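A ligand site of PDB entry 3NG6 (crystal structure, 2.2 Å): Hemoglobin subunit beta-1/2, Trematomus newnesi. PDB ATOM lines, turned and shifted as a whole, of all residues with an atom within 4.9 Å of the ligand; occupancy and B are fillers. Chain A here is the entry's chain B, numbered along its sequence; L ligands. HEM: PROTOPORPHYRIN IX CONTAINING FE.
An oxygen (O2D) of the ligand lies within salt-bridge range of the side-chain amino group of Lys 66.
FE of the ligand is bound by NE2 of His 92, 2.3 Å away.
A ring nitrogen (ND1) of His 92 lies within hydrogen-bond range of the backbone carbonyl oxygen (O) of Leu 88.
OD1 of Asn 102 lies close to OH of Tyr 41 (3.4 Å).
O of Leu 91 is in hydrogen-bond range of N of Leu 96, 3.0 Å away.
The backbone carbonyl oxygen (O) of His 92 lies within hydrogen-bond range of the backbone NH (N) of Val 98, 2.9 Å away.
Residues that only touch the ligand: Thr 38, Tyr 41, Phe 42, His 63, Val 67, Gly 70, Leu 88, Leu 91, Leu 96, Val 98, Asn 102, Phe 103, Leu 106 and Leu 141.
Hydrophobic or aromatic side chains that line the ligand: Tyr 41, Phe 42, His 63, Leu 88, Leu 91, His 92, Leu 96, Val 98, Phe 103, Leu 106 and Leu 141.
Within 4 Å of the ligand: Thr 38, Tyr 41, Phe 42, His 63, Lys 66, Val 67, Gly 70, Leu 88, Leu 91, His 92, Leu 96, Val 98, Asn 102, Phe 103, Leu 106 and Leu 141.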
ATOM      1  N   THR A  38      16.039   6.550   6.583  1.00  0.00           N
ATOM      2  CA  THR A  38      15.537   7.038   5.307  1.00  0.00           C
ATOM      3  C   THR A  38      14.301   7.902   5.489  1.00  0.00           C
ATOM      4  O   THR A  38      13.849   8.548   4.525  1.00  0.00           O
ATOM      5  CB  THR A  38      15.193   5.864   4.356  1.00  0.00           C
ATOM      6  OG1 THR A  38      14.227   5.012   5.000  1.00  0.00           O
ATOM      7  CG2 THR A  38      16.422   5.019   4.068  1.00  0.00           C
ATOM      8  N   TYR A  41      14.140  12.138   4.782  1.00  0.00           N
ATOM      9  CA  TYR A  41      13.861  12.722   3.472  1.00  0.00           C
ATOM     10  C   TYR A  41      12.375  12.874   3.177  1.00  0.00           C
ATOM     11  O   TYR A  41      12.000  13.401   2.125  1.00  0.00           O
ATOM     12  CB  TYR A  41      14.517  11.845   2.390  1.00  0.00           C
ATOM     13  CG  TYR A  41      15.988  11.628   2.661  1.00  0.00           C
ATOM     14  CD1 TYR A  41      16.507  10.363   2.849  1.00  0.00           C
ATOM     15  CD2 TYR A  41      16.867  12.705   2.712  1.00  0.00           C
ATOM     16  CE1 TYR A  41      17.862  10.172   3.087  1.00  0.00           C
ATOM     17  CE2 TYR A  41      18.211  12.531   2.952  1.00  0.00           C
ATOM     18  CZ  TYR A  41      18.705  11.262   3.142  1.00  0.00           C
ATOM     19  OH  TYR A  41      20.062  11.095   3.386  1.00  0.00           O
ATOM     20  N   PHE A  42      11.487  12.442   4.077  1.00  0.00           N
ATOM     21  CA  PHE A  42      10.061  12.525   3.776  1.00  0.00           C
ATOM     22  C   PHE A  42       9.284  13.203   4.892  1.00  0.00           C
ATOM     23  O   PHE A  42       8.298  12.708   5.428  1.00  0.00           O
ATOM     24  CB  PHE A  42       9.533  11.118   3.471  1.00  0.00           C
ATOM     25  CG  PHE A  42      10.297  10.461   2.322  1.00  0.00           C
ATOM     26  CD1 PHE A  42      10.078  10.844   1.013  1.00  0.00           C
ATOM     27  CD2 PHE A  42      11.240   9.476   2.574  1.00  0.00           C
ATOM     28  CE1 PHE A  42      10.776  10.250  -0.030  1.00  0.00           C
ATOM     29  CE2 PHE A  42      11.941   8.881   1.553  1.00  0.00           C
ATOM     30  CZ  PHE A  42      11.711   9.271   0.237  1.00  0.00           C
ATOM     31  N   HIS A  63       4.584   7.818  -3.828  1.00  0.00           N
ATOM     32  CA  HIS A  63       5.980   8.081  -4.157  1.00  0.00           C
ATOM     33  C   HIS A  63       6.743   6.812  -4.512  1.00  0.00           C
ATOM     34  O   HIS A  63       7.651   6.798  -5.354  1.00  0.00           O
ATOM     35  CB  HIS A  63       6.666   8.789  -2.988  1.00  0.00           C
ATOM     36  CG  HIS A  63       8.090   9.116  -3.314  1.00  0.00           C
ATOM     37  ND1 HIS A  63       8.427  10.125  -4.184  1.00  0.00           N
ATOM     38  CD2 HIS A  63       9.248   8.568  -2.912  1.00  0.00           C
ATOM     39  CE1 HIS A  63       9.750  10.205  -4.286  1.00  0.00           C
ATOM     40  NE2 HIS A  63      10.267   9.259  -3.525  1.00  0.00           N
ATOM     41  N   LYS A  66       6.345   5.969  -8.082  1.00  0.00           N
ATOM     42  CA  LYS A  66       7.184   6.958  -8.744  1.00  0.00           C
ATOM     43  C   LYS A  66       8.650   6.550  -8.779  1.00  0.00           C
ATOM     44  O   LYS A  66       9.279   6.579  -9.835  1.00  0.00           O
ATOM     45  CB  LYS A  66       7.046   8.299  -8.026  1.00  0.00           C
ATOM     46  CG  LYS A  66       7.034   9.501  -8.964  1.00  0.00           C
ATOM     47  CD  LYS A  66       7.762  10.687  -8.357  1.00  0.00           C
ATOM     48  CE  LYS A  66       6.940  11.952  -8.545  1.00  0.00           C
ATOM     49  NZ  LYS A  66       7.516  13.121  -7.810  1.00  0.00           N
ATOM     50  N   VAL A  67       9.170   6.182  -7.612  1.00  0.00           N
ATOM     51  CA  VAL A  67      10.552   5.731  -7.434  1.00  0.00           C
ATOM     52  C   VAL A  67      10.846   4.548  -8.351  1.00  0.00           C
ATOM     53  O   VAL A  67      11.872   4.468  -9.022  1.00  0.00           O
ATOM     54  CB  VAL A  67      10.814   5.331  -5.969  1.00  0.00           C
ATOM     55  CG1 VAL A  67      12.022   4.403  -5.885  1.00  0.00           C
ATOM     56  CG2 VAL A  67      11.022   6.562  -5.107  1.00  0.00           C
ATOM     57  N   GLY A  70      11.219   5.375 -12.021  1.00  0.00           N
ATOM     58  CA  GLY A  70      12.501   6.013 -12.219  1.00  0.00           C
ATOM     59  C   GLY A  70      13.544   5.078 -12.803  1.00  0.00           C
ATOM     60  O   GLY A  70      14.518   5.549 -13.398  1.00  0.00           O
ATOM     61  N   LEU A  71      13.325   3.780 -12.629  1.00  0.00           N
ATOM     62  CA  LEU A  71      14.146   2.697 -13.133  1.00  0.00           C
ATOM     63  C   LEU A  71      13.871   2.439 -14.611  1.00  0.00           C
ATOM     64  O   LEU A  71      14.708   1.942 -15.357  1.00  0.00           O
ATOM     65  CB  LEU A  71      13.853   1.399 -12.384  1.00  0.00           C
ATOM     66  CG  LEU A  71      14.260   1.266 -10.913  1.00  0.00           C
ATOM     67  CD1 LEU A  71      13.853  -0.102 -10.365  1.00  0.00           C
ATOM     68  CD2 LEU A  71      15.760   1.485 -10.761  1.00  0.00           C
ATOM     69  N   ARG A  73      13.677   4.173 -17.281  1.00  0.00           N
ATOM     70  CA  ARG A  73      14.651   4.613 -18.292  1.00  0.00           C
ATOM     71  C   ARG A  73      15.828   3.654 -18.394  1.00  0.00           C
ATOM     72  O   ARG A  73      16.365   3.390 -19.469  1.00  0.00           O
ATOM     73  CB  ARG A  73      15.143   6.020 -17.978  1.00  0.00           C
ATOM     74  CG  ARG A  73      15.518   6.298 -16.539  1.00  0.00           C
ATOM     75  CD  ARG A  73      15.839   7.779 -16.343  1.00  0.00           C
ATOM     76  NE  ARG A  73      14.660   8.518 -15.917  1.00  0.00           N
ATOM     77  CZ  ARG A  73      14.567   9.741 -15.444  1.00  0.00           C
ATOM     78  NH1 ARG A  73      15.638  10.508 -15.279  1.00  0.00           N
ATOM     79  NH2 ARG A  73      13.365  10.182 -15.122  1.00  0.00           N
ATOM     80  N   TYR A  85      20.789   8.574 -16.252  1.00  0.00           N
ATOM     81  CA  TYR A  85      20.435   9.099 -14.932  1.00  0.00           C
ATOM     82  C   TYR A  85      21.181  10.378 -14.594  1.00  0.00           C
ATOM     83  O   TYR A  85      21.299  10.741 -13.415  1.00  0.00           O
ATOM     84  CB  TYR A  85      20.668   8.020 -13.868  1.00  0.00           C
ATOM     85  CG  TYR A  85      19.513   7.032 -13.838  1.00  0.00           C
ATOM     86  CD1 TYR A  85      18.312   7.329 -13.211  1.00  0.00           C
ATOM     87  CD2 TYR A  85      19.645   5.792 -14.447  1.00  0.00           C
ATOM     88  CE1 TYR A  85      17.274   6.405 -13.193  1.00  0.00           C
ATOM     89  CE2 TYR A  85      18.609   4.871 -14.443  1.00  0.00           C
ATOM     90  CZ  TYR A  85      17.427   5.190 -13.809  1.00  0.00           C
ATOM     91  OH  TYR A  85      16.396   4.271 -13.795  1.00  0.00           O
ATOM     92  N   LEU A  88      18.608  12.933 -12.726  1.00  0.00           N
ATOM     93  CA  LEU A  88      18.184  12.500 -11.398  1.00  0.00           C
ATOM     94  C   LEU A  88      19.354  12.503 -10.414  1.00  0.00           C
ATOM     95  O   LEU A  88      19.213  12.885  -9.254  1.00  0.00           O
ATOM     96  CB  LEU A  88      17.533  11.127 -11.451  1.00  0.00           C
ATOM     97  CG  LEU A  88      16.001  11.157 -11.289  1.00  0.00           C
ATOM     98  CD1 LEU A  88      15.483   9.828 -10.756  1.00  0.00           C
ATOM     99  CD2 LEU A  88      15.612  12.305 -10.379  1.00  0.00           C
ATOM    100  N   LEU A  91      19.515  15.893  -9.598  1.00  0.00           N
ATOM    101  CA  LEU A  91      18.402  16.236  -8.715  1.00  0.00           C
ATOM    102  C   LEU A  91      18.639  15.742  -7.296  1.00  0.00           C
ATOM    103  O   LEU A  91      18.415  16.451  -6.319  1.00  0.00           O
ATOM    104  CB  LEU A  91      17.078  15.636  -9.209  1.00  0.00           C
ATOM    105  CG  LEU A  91      15.899  15.869  -8.249  1.00  0.00           C
ATOM    106  CD1 LEU A  91      15.407  17.306  -8.351  1.00  0.00           C
ATOM    107  CD2 LEU A  91      14.761  14.896  -8.527  1.00  0.00           C
ATOM    108  N   HIS A  92      19.087  14.491  -7.189  1.00  0.00           N
ATOM    109  CA  HIS A  92      19.187  13.843  -5.890  1.00  0.00           C
ATOM    110  C   HIS A  92      20.288  14.396  -5.007  1.00  0.00           C
ATOM    111  O   HIS A  92      20.156  14.432  -3.783  1.00  0.00           O
ATOM    112  CB  HIS A  92      19.380  12.330  -6.104  1.00  0.00           C
ATOM    113  CG  HIS A  92      18.068  11.663  -6.377  1.00  0.00           C
ATOM    114  ND1 HIS A  92      17.629  11.371  -7.646  1.00  0.00           N
ATOM    115  CD2 HIS A  92      17.094  11.231  -5.533  1.00  0.00           C
ATOM    116  CE1 HIS A  92      16.449  10.778  -7.577  1.00  0.00           C
ATOM    117  NE2 HIS A  92      16.102  10.684  -6.303  1.00  0.00           N
ATOM    118  N   LEU A  96      17.905  17.600  -3.569  1.00  0.00           N
ATOM    119  CA  LEU A  96      17.309  16.851  -2.467  1.00  0.00           C
ATOM    120  C   LEU A  96      18.313  16.498  -1.373  1.00  0.00           C
ATOM    121  O   LEU A  96      17.904  16.218  -0.244  1.00  0.00           O
ATOM    122  CB  LEU A  96      16.643  15.578  -3.019  1.00  0.00           C
ATOM    123  CG  LEU A  96      15.750  15.804  -4.242  1.00  0.00           C
ATOM    124  CD1 LEU A  96      15.424  14.487  -4.921  1.00  0.00           C
ATOM    125  CD2 LEU A  96      14.488  16.553  -3.840  1.00  0.00           C
ATOM    126  N   VAL A  98      20.325  13.830  -0.906  1.00  0.00           N
ATOM    127  CA  VAL A  98      20.123  12.467  -0.408  1.00  0.00           C
ATOM    128  C   VAL A  98      21.409  11.662  -0.350  1.00  0.00           C
ATOM    129  O   VAL A  98      22.150  11.538  -1.328  1.00  0.00           O
ATOM    130  CB  VAL A  98      19.109  11.733  -1.309  1.00  0.00           C
ATOM    131  CG1 VAL A  98      19.058  10.258  -0.966  1.00  0.00           C
ATOM    132  CG2 VAL A  98      17.739  12.379  -1.187  1.00  0.00           C
ATOM    133  N   ASN A 102      21.565   5.206   0.544  1.00  0.00           N
ATOM    134  CA  ASN A 102      20.157   4.827   0.612  1.00  0.00           C
ATOM    135  C   ASN A 102      19.689   4.200  -0.690  1.00  0.00           C
ATOM    136  O   ASN A 102      18.682   3.475  -0.690  1.00  0.00           O
ATOM    137  CB  ASN A 102      19.282   6.041   0.939  1.00  0.00           C
ATOM    138  CG  ASN A 102      19.611   6.631   2.308  1.00  0.00           C
ATOM    139  OD1 ASN A 102      19.668   7.855   2.481  1.00  0.00           O
ATOM    140  ND2 ASN A 102      19.840   5.752   3.268  1.00  0.00           N
ATOM    141  N   PHE A 103      20.407   4.478  -1.774  1.00  0.00           N
ATOM    142  CA  PHE A 103      20.052   3.947  -3.083  1.00  0.00           C
ATOM    143  C   PHE A 103      20.143   2.423  -3.059  1.00  0.00           C
ATOM    144  O   PHE A 103      19.322   1.736  -3.659  1.00  0.00           O
ATOM    145  CB  PHE A 103      20.942   4.512  -4.182  1.00  0.00           C
ATOM    146  CG  PHE A 103      20.705   5.989  -4.464  1.00  0.00           C
ATOM    147  CD1 PHE A 103      19.439   6.519  -4.316  1.00  0.00           C
ATOM    148  CD2 PHE A 103      21.743   6.818  -4.862  1.00  0.00           C
ATOM    149  CE1 PHE A 103      19.205   7.863  -4.568  1.00  0.00           C
ATOM    150  CE2 PHE A 103      21.518   8.156  -5.107  1.00  0.00           C
ATOM    151  CZ  PHE A 103      20.246   8.681  -4.953  1.00  0.00           C
ATOM    152  N   LEU A 106      17.303   0.789  -0.529  1.00  0.00           N
ATOM    153  CA  LEU A 106      16.018   0.714  -1.217  1.00  0.00           C
ATOM    154  C   LEU A 106      16.067  -0.273  -2.369  1.00  0.00           C
ATOM    155  O   LEU A 106      15.093  -0.943  -2.732  1.00  0.00           O
ATOM    156  CB  LEU A 106      15.642   2.127  -1.688  1.00  0.00           C
ATOM    157  CG  LEU A 106      14.328   2.279  -2.448  1.00  0.00           C
ATOM    158  CD1 LEU A 106      13.146   1.868  -1.571  1.00  0.00           C
ATOM    159  CD2 LEU A 106      14.162   3.699  -2.959  1.00  0.00           C
ATOM    160  N   SER A 107      17.240  -0.410  -2.994  1.00  0.00           N
ATOM    161  CA  SER A 107      17.440  -1.357  -4.078  1.00  0.00           C
ATOM    162  C   SER A 107      17.208  -2.778  -3.560  1.00  0.00           C
ATOM    163  O   SER A 107      16.620  -3.632  -4.220  1.00  0.00           O
ATOM    164  CB  SER A 107      18.845  -1.258  -4.669  1.00  0.00           C
ATOM    165  OG  SER A 107      19.079   0.007  -5.257  1.00  0.00           O
ATOM    166  N   ILE A 110      13.508  -3.336  -2.815  1.00  0.00           N
ATOM    167  CA  ILE A 110      12.875  -3.593  -4.098  1.00  0.00           C
ATOM    168  C   ILE A 110      13.138  -5.038  -4.499  1.00  0.00           C
ATOM    169  O   ILE A 110      12.254  -5.771  -4.958  1.00  0.00           O
ATOM    170  CB  ILE A 110      13.380  -2.621  -5.164  1.00  0.00           C
ATOM    171  CG1 ILE A 110      12.975  -1.166  -4.884  1.00  0.00           C
ATOM    172  CG2 ILE A 110      12.938  -3.054  -6.552  1.00  0.00           C
ATOM    173  CD1 ILE A 110      13.941  -0.144  -5.462  1.00  0.00           C
ATOM    174  N   VAL A 137      22.186   0.955 -11.839  1.00  0.00           N
ATOM    175  CA  VAL A 137      21.375   2.156 -11.652  1.00  0.00           C
ATOM    176  C   VAL A 137      21.823   2.921 -10.418  1.00  0.00           C
ATOM    177  O   VAL A 137      21.793   4.149 -10.337  1.00  0.00           O
ATOM    178  CB  VAL A 137      19.883   1.780 -11.559  1.00  0.00           C
ATOM    179  CG1 VAL A 137      19.107   2.737 -10.675  1.00  0.00           C
ATOM    180  CG2 VAL A 137      19.291   1.765 -12.959  1.00  0.00           C
ATOM    181  N   LEU A 141      23.106   6.813 -10.088  1.00  0.00           N
ATOM    182  CA  LEU A 141      22.443   7.782  -9.213  1.00  0.00           C
ATOM    183  C   LEU A 141      23.433   8.621  -8.416  1.00  0.00           C
ATOM    184  O   LEU A 141      23.202   9.808  -8.162  1.00  0.00           O
ATOM    185  CB  LEU A 141      21.488   7.053  -8.262  1.00  0.00           C
ATOM    186  CG  LEU A 141      20.058   6.862  -8.756  1.00  0.00           C
ATOM    187  CD1 LEU A 141      19.336   5.817  -7.913  1.00  0.00           C
ATOM    188  CD2 LEU A 141      19.307   8.192  -8.730  1.00  0.00           C
HETATM  189  CHA HEM L   1      12.395  11.935  -6.100  1.00  0.00           C
HETATM  190  CHB HEM L   1      13.993   8.022  -8.438  1.00  0.00           C
HETATM  191  CHC HEM L   1      16.077   6.452  -4.379  1.00  0.00           C
HETATM  192  CHD HEM L   1      14.593  10.416  -2.072  1.00  0.00           C
HETATM  193  C1A HEM L   1      12.586  10.979  -7.071  1.00  0.00           C
HETATM  194  C2A HEM L   1      11.990  10.974  -8.388  1.00  0.00           C
HETATM  195  C3A HEM L   1      12.408   9.882  -9.033  1.00  0.00           C
HETATM  196  C4A HEM L   1      13.302   9.177  -8.134  1.00  0.00           C
HETATM  197  CMA HEM L   1      12.111   9.415 -10.473  1.00  0.00           C
HETATM  198  CAA HEM L   1      11.065  12.098  -8.907  1.00  0.00           C
HETATM  199  CBA HEM L   1      11.702  13.167  -9.801  1.00  0.00           C
HETATM  200  CGA HEM L   1      10.916  14.433  -9.999  1.00  0.00           C
HETATM  201  O1A HEM L   1       9.798  14.515  -9.429  1.00  0.00           O
HETATM  202  O2A HEM L   1      11.440  15.314 -10.724  1.00  0.00           O
HETATM  203  C1B HEM L   1      14.719   7.261  -7.547  1.00  0.00           C
HETATM  204  C2B HEM L   1      15.383   6.006  -7.848  1.00  0.00           C
HETATM  205  C3B HEM L   1      15.924   5.549  -6.720  1.00  0.00           C
HETATM  206  C4B HEM L   1      15.657   6.533  -5.688  1.00  0.00           C
HETATM  207  CMB HEM L   1      15.384   5.377  -9.257  1.00  0.00           C
HETATM  208  CAB HEM L   1      16.780   4.287  -6.482  1.00  0.00           C
HETATM  209  CBB HEM L   1      16.483   3.146  -7.089  1.00  0.00           C
HETATM  210  C1C HEM L   1      15.771   7.344  -3.374  1.00  0.00           C
HETATM  211  C2C HEM L   1      16.034   7.151  -1.959  1.00  0.00           C
HETATM  212  C3C HEM L   1      15.618   8.247  -1.327  1.00  0.00           C
HETATM  213  C4C HEM L   1      15.116   9.173  -2.318  1.00  0.00           C
HETATM  214  CMC HEM L   1      16.667   5.854  -1.417  1.00  0.00           C
HETATM  215  CAC HEM L   1      15.706   8.610   0.176  1.00  0.00           C
HETATM  216  CBC HEM L   1      15.623   7.680   1.116  1.00  0.00           C
HETATM  217  C1D HEM L   1      13.828  11.164  -2.950  1.00  0.00           C
HETATM  218  C2D HEM L   1      13.098  12.362  -2.620  1.00  0.00           C
HETATM  219  C3D HEM L   1      12.494  12.778  -3.737  1.00  0.00           C
HETATM  220  C4D HEM L   1      12.832  11.853  -4.789  1.00  0.00           C
HETATM  221  CMD HEM L   1      13.066  12.981  -1.203  1.00  0.00           C
HETATM  222  CAD HEM L   1      11.590  14.018  -3.943  1.00  0.00           C
HETATM  223  CBD HEM L   1      10.082  13.820  -3.835  1.00  0.00           C
HETATM  224  CGD HEM L   1       9.254  14.514  -4.888  1.00  0.00           C
HETATM  225  O1D HEM L   1       8.915  15.698  -4.665  1.00  0.00           O
HETATM  226  O2D HEM L   1       8.966  13.834  -5.905  1.00  0.00           O
HETATM  227  NA  HEM L   1      13.397   9.856  -6.933  1.00  0.00           N
HETATM  228  NB  HEM L   1      14.894   7.569  -6.211  1.00  0.00           N
HETATM  229  NC  HEM L   1      15.200   8.590  -3.573  1.00  0.00           N
HETATM  230  ND  HEM L   1      13.655  10.869  -4.290  1.00  0.00           N
HETATM  231 FE   HEM L   1      14.536   9.381  -5.334  1.00  0.00          FE
